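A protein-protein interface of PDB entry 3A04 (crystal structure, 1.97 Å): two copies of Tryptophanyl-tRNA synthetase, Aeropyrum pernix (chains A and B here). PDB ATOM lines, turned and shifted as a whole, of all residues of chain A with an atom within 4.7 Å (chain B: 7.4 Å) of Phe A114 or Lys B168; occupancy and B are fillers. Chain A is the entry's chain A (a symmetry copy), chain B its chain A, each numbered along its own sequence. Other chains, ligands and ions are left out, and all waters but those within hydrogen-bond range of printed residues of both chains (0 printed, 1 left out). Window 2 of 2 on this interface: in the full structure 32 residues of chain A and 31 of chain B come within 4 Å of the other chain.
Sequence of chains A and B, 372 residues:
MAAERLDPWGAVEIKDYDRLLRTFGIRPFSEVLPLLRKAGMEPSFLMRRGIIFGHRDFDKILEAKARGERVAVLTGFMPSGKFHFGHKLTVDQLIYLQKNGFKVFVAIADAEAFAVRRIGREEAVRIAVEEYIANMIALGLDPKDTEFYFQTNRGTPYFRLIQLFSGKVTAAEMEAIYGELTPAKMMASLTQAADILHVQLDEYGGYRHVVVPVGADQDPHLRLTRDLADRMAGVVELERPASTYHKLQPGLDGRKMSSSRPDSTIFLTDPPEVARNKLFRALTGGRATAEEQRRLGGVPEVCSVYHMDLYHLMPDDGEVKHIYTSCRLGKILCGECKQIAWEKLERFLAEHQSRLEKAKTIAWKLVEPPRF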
ATOM      1  N   ASP A 110     -24.743  15.726 -17.952  1.00  0.00           N
ATOM      2  CA  ASP A 110     -24.488  16.043 -19.344  1.00  0.00           C
ATOM      3  C   ASP A 110     -23.575  15.056 -20.064  1.00  0.00           C
ATOM      4  O   ASP A 110     -23.649  14.938 -21.287  1.00  0.00           O
ATOM      5  CB  ASP A 110     -23.884  17.500 -19.491  1.00  0.00           C
ATOM      6  CG  ASP A 110     -22.425  17.600 -18.981  1.00  0.00           C
ATOM      7  OD1 ASP A 110     -22.103  17.107 -17.854  1.00  0.00           O
ATOM      8  OD2 ASP A 110     -21.563  18.265 -19.669  1.00  0.00           O
ATOM      9  N   ALA A 111     -22.715  14.302 -19.328  1.00  0.00           N
ATOM     10  CA  ALA A 111     -21.925  13.271 -19.951  1.00  0.00           C
ATOM     11  C   ALA A 111     -22.867  12.103 -20.433  1.00  0.00           C
ATOM     12  O   ALA A 111     -22.818  11.630 -21.598  1.00  0.00           O
ATOM     13  CB  ALA A 111     -20.854  12.727 -18.896  1.00  0.00           C
ATOM     14  N   GLU A 112     -23.757  11.694 -19.555  1.00  0.00           N
ATOM     15  CA  GLU A 112     -24.733  10.665 -19.932  1.00  0.00           C
ATOM     16  C   GLU A 112     -25.636  11.153 -21.069  1.00  0.00           C
ATOM     17  O   GLU A 112     -25.945  10.376 -22.022  1.00  0.00           O
ATOM     18  CB  GLU A 112     -25.554  10.252 -18.719  1.00  0.00           C
ATOM     19  CG  GLU A 112     -26.463   9.064 -19.031  1.00  0.00           C
ATOM     20  CD  GLU A 112     -27.268   8.591 -17.801  1.00  0.00           C
ATOM     21  OE1 GLU A 112     -26.930   8.962 -16.638  1.00  0.00           O
ATOM     22  OE2 GLU A 112     -28.185   7.771 -18.025  1.00  0.00           O
ATOM     23  N   ALA A 113     -26.060  12.413 -20.983  1.00  0.00           N
ATOM     24  CA  ALA A 113     -26.916  13.026 -22.035  1.00  0.00           C
ATOM     25  C   ALA A 113     -26.233  12.894 -23.398  1.00  0.00           C
ATOM     26  O   ALA A 113     -26.857  12.498 -24.410  1.00  0.00           O
ATOM     27  CB  ALA A 113     -27.165  14.549 -21.734  1.00  0.00           C
ATOM     28  N   PHE A 114     -24.929  13.197 -23.442  1.00  0.00           N
ATOM     29  CA  PHE A 114     -24.189  13.113 -24.686  1.00  0.00           C
ATOM     30  C   PHE A 114     -24.039  11.652 -25.123  1.00  0.00           C
ATOM     31  O   PHE A 114     -24.391  11.279 -26.259  1.00  0.00           O
ATOM     32  CB  PHE A 114     -22.803  13.773 -24.588  1.00  0.00           C
ATOM     33  CG  PHE A 114     -22.023  13.701 -25.884  1.00  0.00           C
ATOM     34  CD1 PHE A 114     -22.237  14.666 -26.867  1.00  0.00           C
ATOM     35  CD2 PHE A 114     -21.109  12.622 -26.127  1.00  0.00           C
ATOM     36  CE1 PHE A 114     -21.534  14.601 -28.058  1.00  0.00           C
ATOM     37  CE2 PHE A 114     -20.380  12.537 -27.311  1.00  0.00           C
ATOM     38  CZ  PHE A 114     -20.593  13.548 -28.267  1.00  0.00           C
ATOM     39  N   ALA A 115     -23.480  10.828 -24.242  1.00  0.00           N
ATOM     40  CA  ALA A 115     -22.977   9.500 -24.645  1.00  0.00           C
ATOM     41  C   ALA A 115     -24.105   8.463 -24.774  1.00  0.00           C
ATOM     42  O   ALA A 115     -24.071   7.609 -25.667  1.00  0.00           O
ATOM     43  CB  ALA A 115     -21.900   8.984 -23.610  1.00  0.00           C
ATOM     44  N   VAL A 116     -25.096   8.516 -23.903  1.00  0.00           N
ATOM     45  CA  VAL A 116     -26.176   7.515 -23.940  1.00  0.00           C
ATOM     46  C   VAL A 116     -27.311   8.149 -24.788  1.00  0.00           C
ATOM     47  O   VAL A 116     -27.852   7.494 -25.703  1.00  0.00           O
ATOM     48  CB  VAL A 116     -26.714   7.123 -22.538  1.00  0.00           C
ATOM     49  CG1 VAL A 116     -27.941   6.148 -22.636  1.00  0.00           C
ATOM     50  CG2 VAL A 116     -25.631   6.461 -21.690  1.00  0.00           C
ATOM     51  N   ARG A 117     -27.696   9.377 -24.500  1.00  0.00           N
ATOM     52  CA  ARG A 117     -28.965   9.871 -25.150  1.00  0.00           C
ATOM     53  C   ARG A 117     -28.726  10.633 -26.426  1.00  0.00           C
ATOM     54  O   ARG A 117     -29.670  11.091 -27.053  1.00  0.00           O
ATOM     55  CB  ARG A 117     -29.732  10.769 -24.216  1.00  0.00           C
ATOM     56  CG  ARG A 117     -29.980  10.145 -22.884  1.00  0.00           C
ATOM     57  CD  ARG A 117     -31.331   9.516 -22.813  1.00  0.00           C
ATOM     58  NE  ARG A 117     -31.654   9.217 -21.409  1.00  0.00           N
ATOM     59  CZ  ARG A 117     -32.617   9.812 -20.695  1.00  0.00           C
ATOM     60  NH1 ARG A 117     -33.426  10.760 -21.248  1.00  0.00           N
ATOM     61  NH2 ARG A 117     -32.768   9.431 -19.428  1.00  0.00           N
ATOM     62  N   ARG A 118     -27.450  10.842 -26.761  1.00  0.00           N
ATOM     63  CA  ARG A 118     -27.060  11.470 -28.011  1.00  0.00           C
ATOM     64  C   ARG A 118     -27.532  12.898 -28.062  1.00  0.00           C
ATOM     65  O   ARG A 118     -27.886  13.399 -29.109  1.00  0.00           O
ATOM     66  CB  ARG A 118     -27.571  10.675 -29.249  1.00  0.00           C
ATOM     67  CG  ARG A 118     -26.845   9.357 -29.509  1.00  0.00           C
ATOM     68  CD  ARG A 118     -27.555   8.447 -30.613  1.00  0.00           C
ATOM     69  NE  ARG A 118     -28.906   8.083 -30.154  1.00  0.00           N
ATOM     70  CZ  ARG A 118     -30.045   8.259 -30.841  1.00  0.00           C
ATOM     71  NH1 ARG A 118     -30.028   8.745 -32.087  1.00  0.00           N
ATOM     72  NH2 ARG A 118     -31.215   7.927 -30.293  1.00  0.00           N
ATOM     73  N   ILE A 119     -27.538  13.564 -26.925  1.00  0.00           N
ATOM     74  CA  ILE A 119     -27.888  14.977 -26.872  1.00  0.00           C
ATOM     75  C   ILE A 119     -26.642  15.850 -27.046  1.00  0.00           C
ATOM     76  O   ILE A 119     -25.654  15.695 -26.291  1.00  0.00           O
ATOM     77  CB  ILE A 119     -28.557  15.287 -25.541  1.00  0.00           C
ATOM     78  CG1 ILE A 119     -29.908  14.545 -25.489  1.00  0.00           C
ATOM     79  CG2 ILE A 119     -28.804  16.772 -25.336  1.00  0.00           C
ATOM     80  CD1 ILE A 119     -30.466  14.635 -24.090  1.00  0.00           C
ATOM     81  N   ARG A 121     -23.778  18.898 -27.128  1.00  0.00           N
ATOM     82  CA  ARG A 121     -23.130  19.602 -26.020  1.00  0.00           C
ATOM     83  C   ARG A 121     -23.805  20.920 -25.778  1.00  0.00           C
ATOM     84  O   ARG A 121     -24.141  21.270 -24.643  1.00  0.00           O
ATOM     85  CB  ARG A 121     -21.601  19.789 -26.252  1.00  0.00           C
ATOM     86  CG  ARG A 121     -20.927  18.460 -26.560  1.00  0.00           C
ATOM     87  CD  ARG A 121     -20.808  17.544 -25.253  1.00  0.00           C
ATOM     88  NE  ARG A 121     -19.965  18.225 -24.256  1.00  0.00           N
ATOM     89  CZ  ARG A 121     -20.146  18.168 -22.948  1.00  0.00           C
ATOM     90  NH1 ARG A 121     -21.252  17.572 -22.415  1.00  0.00           N
ATOM     91  NH2 ARG A 121     -19.294  18.786 -22.168  1.00  0.00           N
ATOM     92  N   ARG B 160     -12.638  14.562 -19.872  1.00  0.00           N
ATOM     93  CA  ARG B 160     -13.853  14.797 -20.673  1.00  0.00           C
ATOM     94  C   ARG B 160     -13.791  14.043 -22.007  1.00  0.00           C
ATOM     95  O   ARG B 160     -14.805  13.546 -22.510  1.00  0.00           O
ATOM     96  CB  ARG B 160     -14.004  16.289 -20.943  1.00  0.00           C
ATOM     97  CG  ARG B 160     -15.382  16.614 -21.579  1.00  0.00           C
ATOM     98  CD  ARG B 160     -15.558  18.150 -21.750  1.00  0.00           C
ATOM     99  NE  ARG B 160     -15.338  18.908 -20.550  1.00  0.00           N
ATOM    100  CZ  ARG B 160     -14.685  20.064 -20.502  1.00  0.00           C
ATOM    101  NH1 ARG B 160     -14.171  20.587 -21.601  1.00  0.00           N
ATOM    102  NH2 ARG B 160     -14.570  20.695 -19.352  1.00  0.00           N
ATOM    103  N   GLN B 163     -14.965  10.605 -21.322  1.00  0.00           N
ATOM    104  CA  GLN B 163     -16.443  10.571 -21.167  1.00  0.00           C
ATOM    105  C   GLN B 163     -17.209  10.690 -22.506  1.00  0.00           C
ATOM    106  O   GLN B 163     -18.156   9.952 -22.765  1.00  0.00           O
ATOM    107  CB  GLN B 163     -16.899  11.689 -20.280  1.00  0.00           C
ATOM    108  CG  GLN B 163     -16.399  11.615 -18.844  1.00  0.00           C
ATOM    109  CD  GLN B 163     -16.742  12.896 -18.054  1.00  0.00           C
ATOM    110  OE1 GLN B 163     -16.180  13.985 -18.310  1.00  0.00           O
ATOM    111  NE2 GLN B 163     -17.651  12.765 -17.074  1.00  0.00           N
ATOM    112  N   LEU B 164     -16.733  11.540 -23.381  1.00  0.00           N
ATOM    113  CA  LEU B 164     -17.412  11.740 -24.658  1.00  0.00           C
ATOM    114  C   LEU B 164     -17.084  10.599 -25.611  1.00  0.00           C
ATOM    115  O   LEU B 164     -17.958  10.225 -26.371  1.00  0.00           O
ATOM    116  CB  LEU B 164     -17.026  13.075 -25.273  1.00  0.00           C
ATOM    117  CG  LEU B 164     -17.405  14.286 -24.362  1.00  0.00           C
ATOM    118  CD1 LEU B 164     -17.054  15.585 -25.137  1.00  0.00           C
ATOM    119  CD2 LEU B 164     -18.855  14.334 -23.945  1.00  0.00           C
ATOM    120  N   PHE B 165     -15.861  10.012 -25.542  1.00  0.00           N
ATOM    121  CA  PHE B 165     -15.536   8.882 -26.406  1.00  0.00           C
ATOM    122  C   PHE B 165     -16.447   7.709 -26.137  1.00  0.00           C
ATOM    123  O   PHE B 165     -16.689   6.907 -27.070  1.00  0.00           O
ATOM    124  CB  PHE B 165     -14.096   8.346 -26.227  1.00  0.00           C
ATOM    125  CG  PHE B 165     -13.015   9.301 -26.664  1.00  0.00           C
ATOM    126  CD1 PHE B 165     -13.285  10.388 -27.494  1.00  0.00           C
ATOM    127  CD2 PHE B 165     -11.674   9.049 -26.298  1.00  0.00           C
ATOM    128  CE1 PHE B 165     -12.260  11.273 -27.917  1.00  0.00           C
ATOM    129  CE2 PHE B 165     -10.634   9.930 -26.724  1.00  0.00           C
ATOM    130  CZ  PHE B 165     -10.930  11.040 -27.538  1.00  0.00           C
ATOM    131  N   SER B 166     -16.899   7.528 -24.887  1.00  0.00           N
ATOM    132  CA  SER B 166     -17.724   6.349 -24.564  1.00  0.00           C
ATOM    133  C   SER B 166     -19.028   6.304 -25.351  1.00  0.00           C
ATOM    134  O   SER B 166     -19.594   5.199 -25.528  1.00  0.00           O
ATOM    135  CB  SER B 166     -18.030   6.274 -23.068  1.00  0.00           C
ATOM    136  OG  SER B 166     -18.965   7.275 -22.702  1.00  0.00           O
ATOM    137  N   GLY B 167     -19.440   7.445 -25.905  1.00  0.00           N
ATOM    138  CA  GLY B 167     -20.649   7.467 -26.757  1.00  0.00           C
ATOM    139  C   GLY B 167     -20.372   7.118 -28.227  1.00  0.00           C
ATOM    140  O   GLY B 167     -21.311   6.936 -29.010  1.00  0.00           O
ATOM    141  N   LYS B 168     -19.102   6.951 -28.583  1.00  0.00           N
ATOM    142  CA  LYS B 168     -18.742   6.830 -30.002  1.00  0.00           C
ATOM    143  C   LYS B 168     -18.074   5.525 -30.374  1.00  0.00           C
ATOM    144  O   LYS B 168     -17.421   5.422 -31.387  1.00  0.00           O
ATOM    145  CB  LYS B 168     -17.875   8.008 -30.420  1.00  0.00           C
ATOM    146  CG  LYS B 168     -18.534   9.387 -30.187  1.00  0.00           C
ATOM    147  CD  LYS B 168     -19.734   9.533 -31.145  1.00  0.00           C
ATOM    148  CE  LYS B 168     -20.172  10.981 -31.173  1.00  0.00           C
ATOM    149  NZ  LYS B 168     -21.403  11.078 -32.043  1.00  0.00           N
ATOM    150  N   VAL B 169     -18.239   4.520 -29.550  1.00  0.00           N
ATOM    151  CA  VAL B 169     -17.713   3.230 -29.867  1.00  0.00           C
ATOM    152  C   VAL B 169     -18.712   2.193 -29.350  1.00  0.00           C
ATOM    153  O   VAL B 169     -19.371   2.431 -28.338  1.00  0.00           O
ATOM    154  CB  VAL B 169     -16.279   3.097 -29.257  1.00  0.00           C
ATOM    155  CG1 VAL B 169     -16.300   3.271 -27.743  1.00  0.00           C
ATOM    156  CG2 VAL B 169     -15.632   1.769 -29.685  1.00  0.00           C
ATOM    157  N   THR B 170     -18.846   1.057 -30.049  1.00  0.00           N
ATOM    158  CA  THR B 170     -19.729  -0.031 -29.579  1.00  0.00           C
ATOM    159  C   THR B 170     -18.966  -1.078 -28.752  1.00  0.00           C
ATOM    160  O   THR B 170     -17.747  -1.180 -28.824  1.00  0.00           O
ATOM    161  CB  THR B 170     -20.421  -0.755 -30.805  1.00  0.00           C
ATOM    162  OG1 THR B 170     -19.404  -1.385 -31.577  1.00  0.00           O
ATOM    163  CG2 THR B 170     -21.114   0.261 -31.675  1.00  0.00           C
ATOM    164  N   GLU B 173     -17.051  -3.315 -31.291  1.00  0.00           N
ATOM    165  CA  GLU B 173     -15.764  -2.741 -31.680  1.00  0.00           C
ATOM    166  C   GLU B 173     -14.679  -2.979 -30.637  1.00  0.00           C
ATOM    167  O   GLU B 173     -13.575  -3.382 -30.957  1.00  0.00           O
ATOM    168  CB  GLU B 173     -15.924  -1.252 -31.927  1.00  0.00           C
ATOM    169  CG  GLU B 173     -16.799  -0.980 -33.151  1.00  0.00           C
ATOM    170  CD  GLU B 173     -16.915   0.499 -33.446  1.00  0.00           C
ATOM    171  OE1 GLU B 173     -17.374   1.262 -32.582  1.00  0.00           O
ATOM    172  OE2 GLU B 173     -16.554   0.891 -34.562  1.00  0.00           O
ATOM    173  N   MET B 174     -14.995  -2.722 -29.382  1.00  0.00           N
ATOM    174  CA  MET B 174     -14.001  -2.914 -28.357  1.00  0.00           C
ATOM    175  C   MET B 174     -13.661  -4.382 -28.179  1.00  0.00           C
ATOM    176  O   MET B 174     -12.491  -4.738 -28.125  1.00  0.00           O
ATOM    177  CB  MET B 174     -14.512  -2.326 -27.057  1.00  0.00           C
ATOM    178  CG  MET B 174     -14.538  -0.838 -27.038  1.00  0.00           C
ATOM    179  SD  MET B 174     -14.926  -0.483 -25.299  1.00  0.00           S
ATOM    180  CE  MET B 174     -14.983   1.227 -25.381  1.00  0.00           C
ATOM    181  N   LEU B 190     -10.710   3.359 -23.753  1.00  0.00           N
ATOM    182  CA  LEU B 190     -11.013   4.802 -23.950  1.00  0.00           C
ATOM    183  C   LEU B 190      -9.887   5.687 -23.413  1.00  0.00           C
ATOM    184  O   LEU B 190      -9.602   6.738 -23.975  1.00  0.00           O
ATOM    185  CB  LEU B 190     -12.318   5.226 -23.253  1.00  0.00           C
ATOM    186  CG  LEU B 190     -13.607   4.439 -23.593  1.00  0.00           C
ATOM    187  CD1 LEU B 190     -14.782   4.825 -22.685  1.00  0.00           C
ATOM    188  CD2 LEU B 190     -14.017   4.668 -25.013  1.00  0.00           C
ATOM    189  N   LEU B 224      -8.786   2.248 -33.772  1.00  0.00           N
ATOM    190  CA  LEU B 224      -9.992   2.662 -33.054  1.00  0.00           C
ATOM    191  C   LEU B 224      -9.810   4.150 -32.595  1.00  0.00           C
ATOM    192  O   LEU B 224     -10.733   4.944 -32.690  1.00  0.00           O
ATOM    193  CB  LEU B 224     -10.299   1.768 -31.850  1.00  0.00           C
ATOM    194  CG  LEU B 224     -11.418   2.240 -30.899  1.00  0.00           C
ATOM    195  CD1 LEU B 224     -12.798   2.229 -31.646  1.00  0.00           C
ATOM    196  CD2 LEU B 224     -11.501   1.384 -29.583  1.00  0.00           C
ATOM    197  N   ASP B 227     -10.417   6.321 -35.526  1.00  0.00           N
ATOM    198  CA  ASP B 227     -11.900   6.438 -35.670  1.00  0.00           C
ATOM    199  C   ASP B 227     -12.539   7.399 -34.658  1.00  0.00           C
ATOM    200  O   ASP B 227     -13.396   8.183 -35.023  1.00  0.00           O
ATOM    201  CB  ASP B 227     -12.627   5.124 -35.604  1.00  0.00           C
ATOM    202  CG  ASP B 227     -12.249   4.189 -36.784  1.00  0.00           C
ATOM    203  OD1 ASP B 227     -11.680   4.663 -37.774  1.00  0.00           O
ATOM    204  OD2 ASP B 227     -12.378   2.953 -36.630  1.00  0.00           O
ATOM    205  N   LEU B 228     -12.176   7.278 -33.383  1.00  0.00           N
ATOM    206  CA  LEU B 228     -12.643   8.207 -32.378  1.00  0.00           C
ATOM    207  C   LEU B 228     -12.352   9.683 -32.758  1.00  0.00           C
ATOM    208  O   LEU B 228     -13.260  10.553 -32.667  1.00  0.00           O
ATOM    209  CB  LEU B 228     -12.144   7.815 -30.946  1.00  0.00           C
ATOM    210  CG  LEU B 228     -12.830   6.629 -30.279  1.00  0.00           C
ATOM    211  CD1 LEU B 228     -11.926   6.232 -29.056  1.00  0.00           C
ATOM    212  CD2 LEU B 228     -14.283   7.079 -29.800  1.00  0.00           C
ATOM    213  N   ARG B 231     -14.885  10.546 -35.403  1.00  0.00           N
ATOM    214  CA  ARG B 231     -16.253  10.522 -34.807  1.00  0.00           C
ATOM    215  C   ARG B 231     -16.512  11.696 -33.855  1.00  0.00           C
ATOM    216  O   ARG B 231     -17.684  12.031 -33.566  1.00  0.00           O
ATOM    217  CB  ARG B 231     -16.545   9.191 -34.136  1.00  0.00           C
ATOM    218  CG  ARG B 231     -16.631   8.011 -35.151  1.00  0.00           C
ATOM    219  CD  ARG B 231     -16.609   6.695 -34.387  1.00  0.00           C
ATOM    220  NE  ARG B 231     -16.420   5.598 -35.312  1.00  0.00           N
ATOM    221  CZ  ARG B 231     -16.465   4.317 -34.991  1.00  0.00           C
ATOM    222  NH1 ARG B 231     -16.674   3.906 -33.726  1.00  0.00           N
ATOM    223  NH2 ARG B 231     -16.316   3.422 -35.955  1.00  0.00           N
ATOM    224  N   MET B 232     -15.466  12.361 -33.397  1.00  0.00           N
ATOM    225  CA  MET B 232     -15.659  13.551 -32.586  1.00  0.00           C
ATOM    226  C   MET B 232     -15.899  14.819 -33.408  1.00  0.00           C
ATOM    227  O   MET B 232     -16.067  15.876 -32.840  1.00  0.00           O
ATOM    228  CB  MET B 232     -14.484  13.774 -31.596  1.00  0.00           C
ATOM    229  CG  MET B 232     -14.431  12.641 -30.488  1.00  0.00           C
ATOM    230  SD  MET B 232     -15.929  12.684 -29.437  1.00  0.00           S
ATOM    231  CE  MET B 232     -15.287  14.114 -28.673  1.00  0.00           C
ATOM    232  N   ALA B 233     -15.820  14.760 -34.744  1.00  0.00           N
ATOM    233  CA  ALA B 233     -16.032  16.012 -35.546  1.00  0.00           C
ATOM    234  C   ALA B 233     -17.327  16.773 -35.153  1.00  0.00           C
ATOM    235  O   ALA B 233     -18.337  16.167 -34.986  1.00  0.00           O
ATOM    236  CB  ALA B 233     -16.013  15.695 -37.094  1.00  0.00           C
ATOM    237  N   GLY B 234     -17.281  18.074 -34.936  1.00  0.00           N
ATOM    238  CA  GLY B 234     -18.468  18.776 -34.476  1.00  0.00           C
ATOM    239  C   GLY B 234     -18.508  18.981 -32.956  1.00  0.00           C
ATOM    240  O   GLY B 234     -19.279  19.806 -32.426  1.00  0.00           O
ATOM    241  N   VAL B 235     -17.706  18.203 -32.239  1.00  0.00           N
ATOM    242  CA  VAL B 235     -17.645  18.282 -30.801  1.00  0.00           C
ATOM    243  C   VAL B 235     -16.307  18.804 -30.392  1.00  0.00           C
ATOM    244  O   VAL B 235     -16.226  19.795 -29.686  1.00  0.00           O
ATOM    245  CB  VAL B 235     -17.864  16.866 -30.236  1.00  0.00           C
ATOM    246  CG1 VAL B 235     -17.970  16.895 -28.774  1.00  0.00           C
ATOM    247  CG2 VAL B 235     -19.092  16.314 -30.845  1.00  0.00           C
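The backbone carbonyl oxygen (O) of Lys B168 sits at hydrogen-bond distance from the guanidinium group (NH1) of Arg B231, at 2.9 Å. The side-chain carboxylate of Asp A110 is in salt-bridge range of the guanidinium group of Arg A121, 2.8 Å away. O of Gln B163 is in hydrogen-bond range of OG of Ser B166 (2.8 Å).
Phe A114 touches just these residues of chain B: Leu B164 and Lys B168. Printed residues of chain B within 4 Å of Ala A115: Gln B163, Ser B166 and Gly B167. Of the printed residues of chain B, Arg A121 touches Arg B160 and Leu B164. Of the printed residues of chain A, Arg B160 touches Arg A121. Of the printed residues of chain A, Ser B166 touches Ala A115. Of the printed residues of chain A, Gly B167 touches Ala A115 (3.6 Å). Printed residues of chain A within 4 Å of Lys B168: Phe A114. Gly B234 touches none of the printed residues of chain A. The nearest residue of chain B that does not touch Phe A114 is Val B235 (4.1 Å). The nearest printed residue of chain A that does not touch Lys B168 is Ala A115 (5.8 Å).
Among the printed residues, pairs that only touch across the chains: Ala A111 with Gln B163, Phe A114 with Leu B164, Phe A114 with Lys B168, Ala A115 with Gln B163, Ala A115 with Ser B166, Ala A115 with Gly B167, Arg A121 with Arg B160 and Arg A121 with Leu B164.
No position is printed for both chains. Of the 8 pairs that touch across the chains among the printed residues, none has its exchanged pair printed and touching as well.
Along chain B the printed residues that touch a printed residue of chain A span positions 160 to 168. Of the 11 printed residues of chain A, 4 touch a printed residue of chain B. Among the printed residues, 8 pairs touch across the chains. Among the printed residues, no Asp or Glu carboxylate lies within 4 Å of a Lys or Arg side-chain nitrogen of the other chain.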
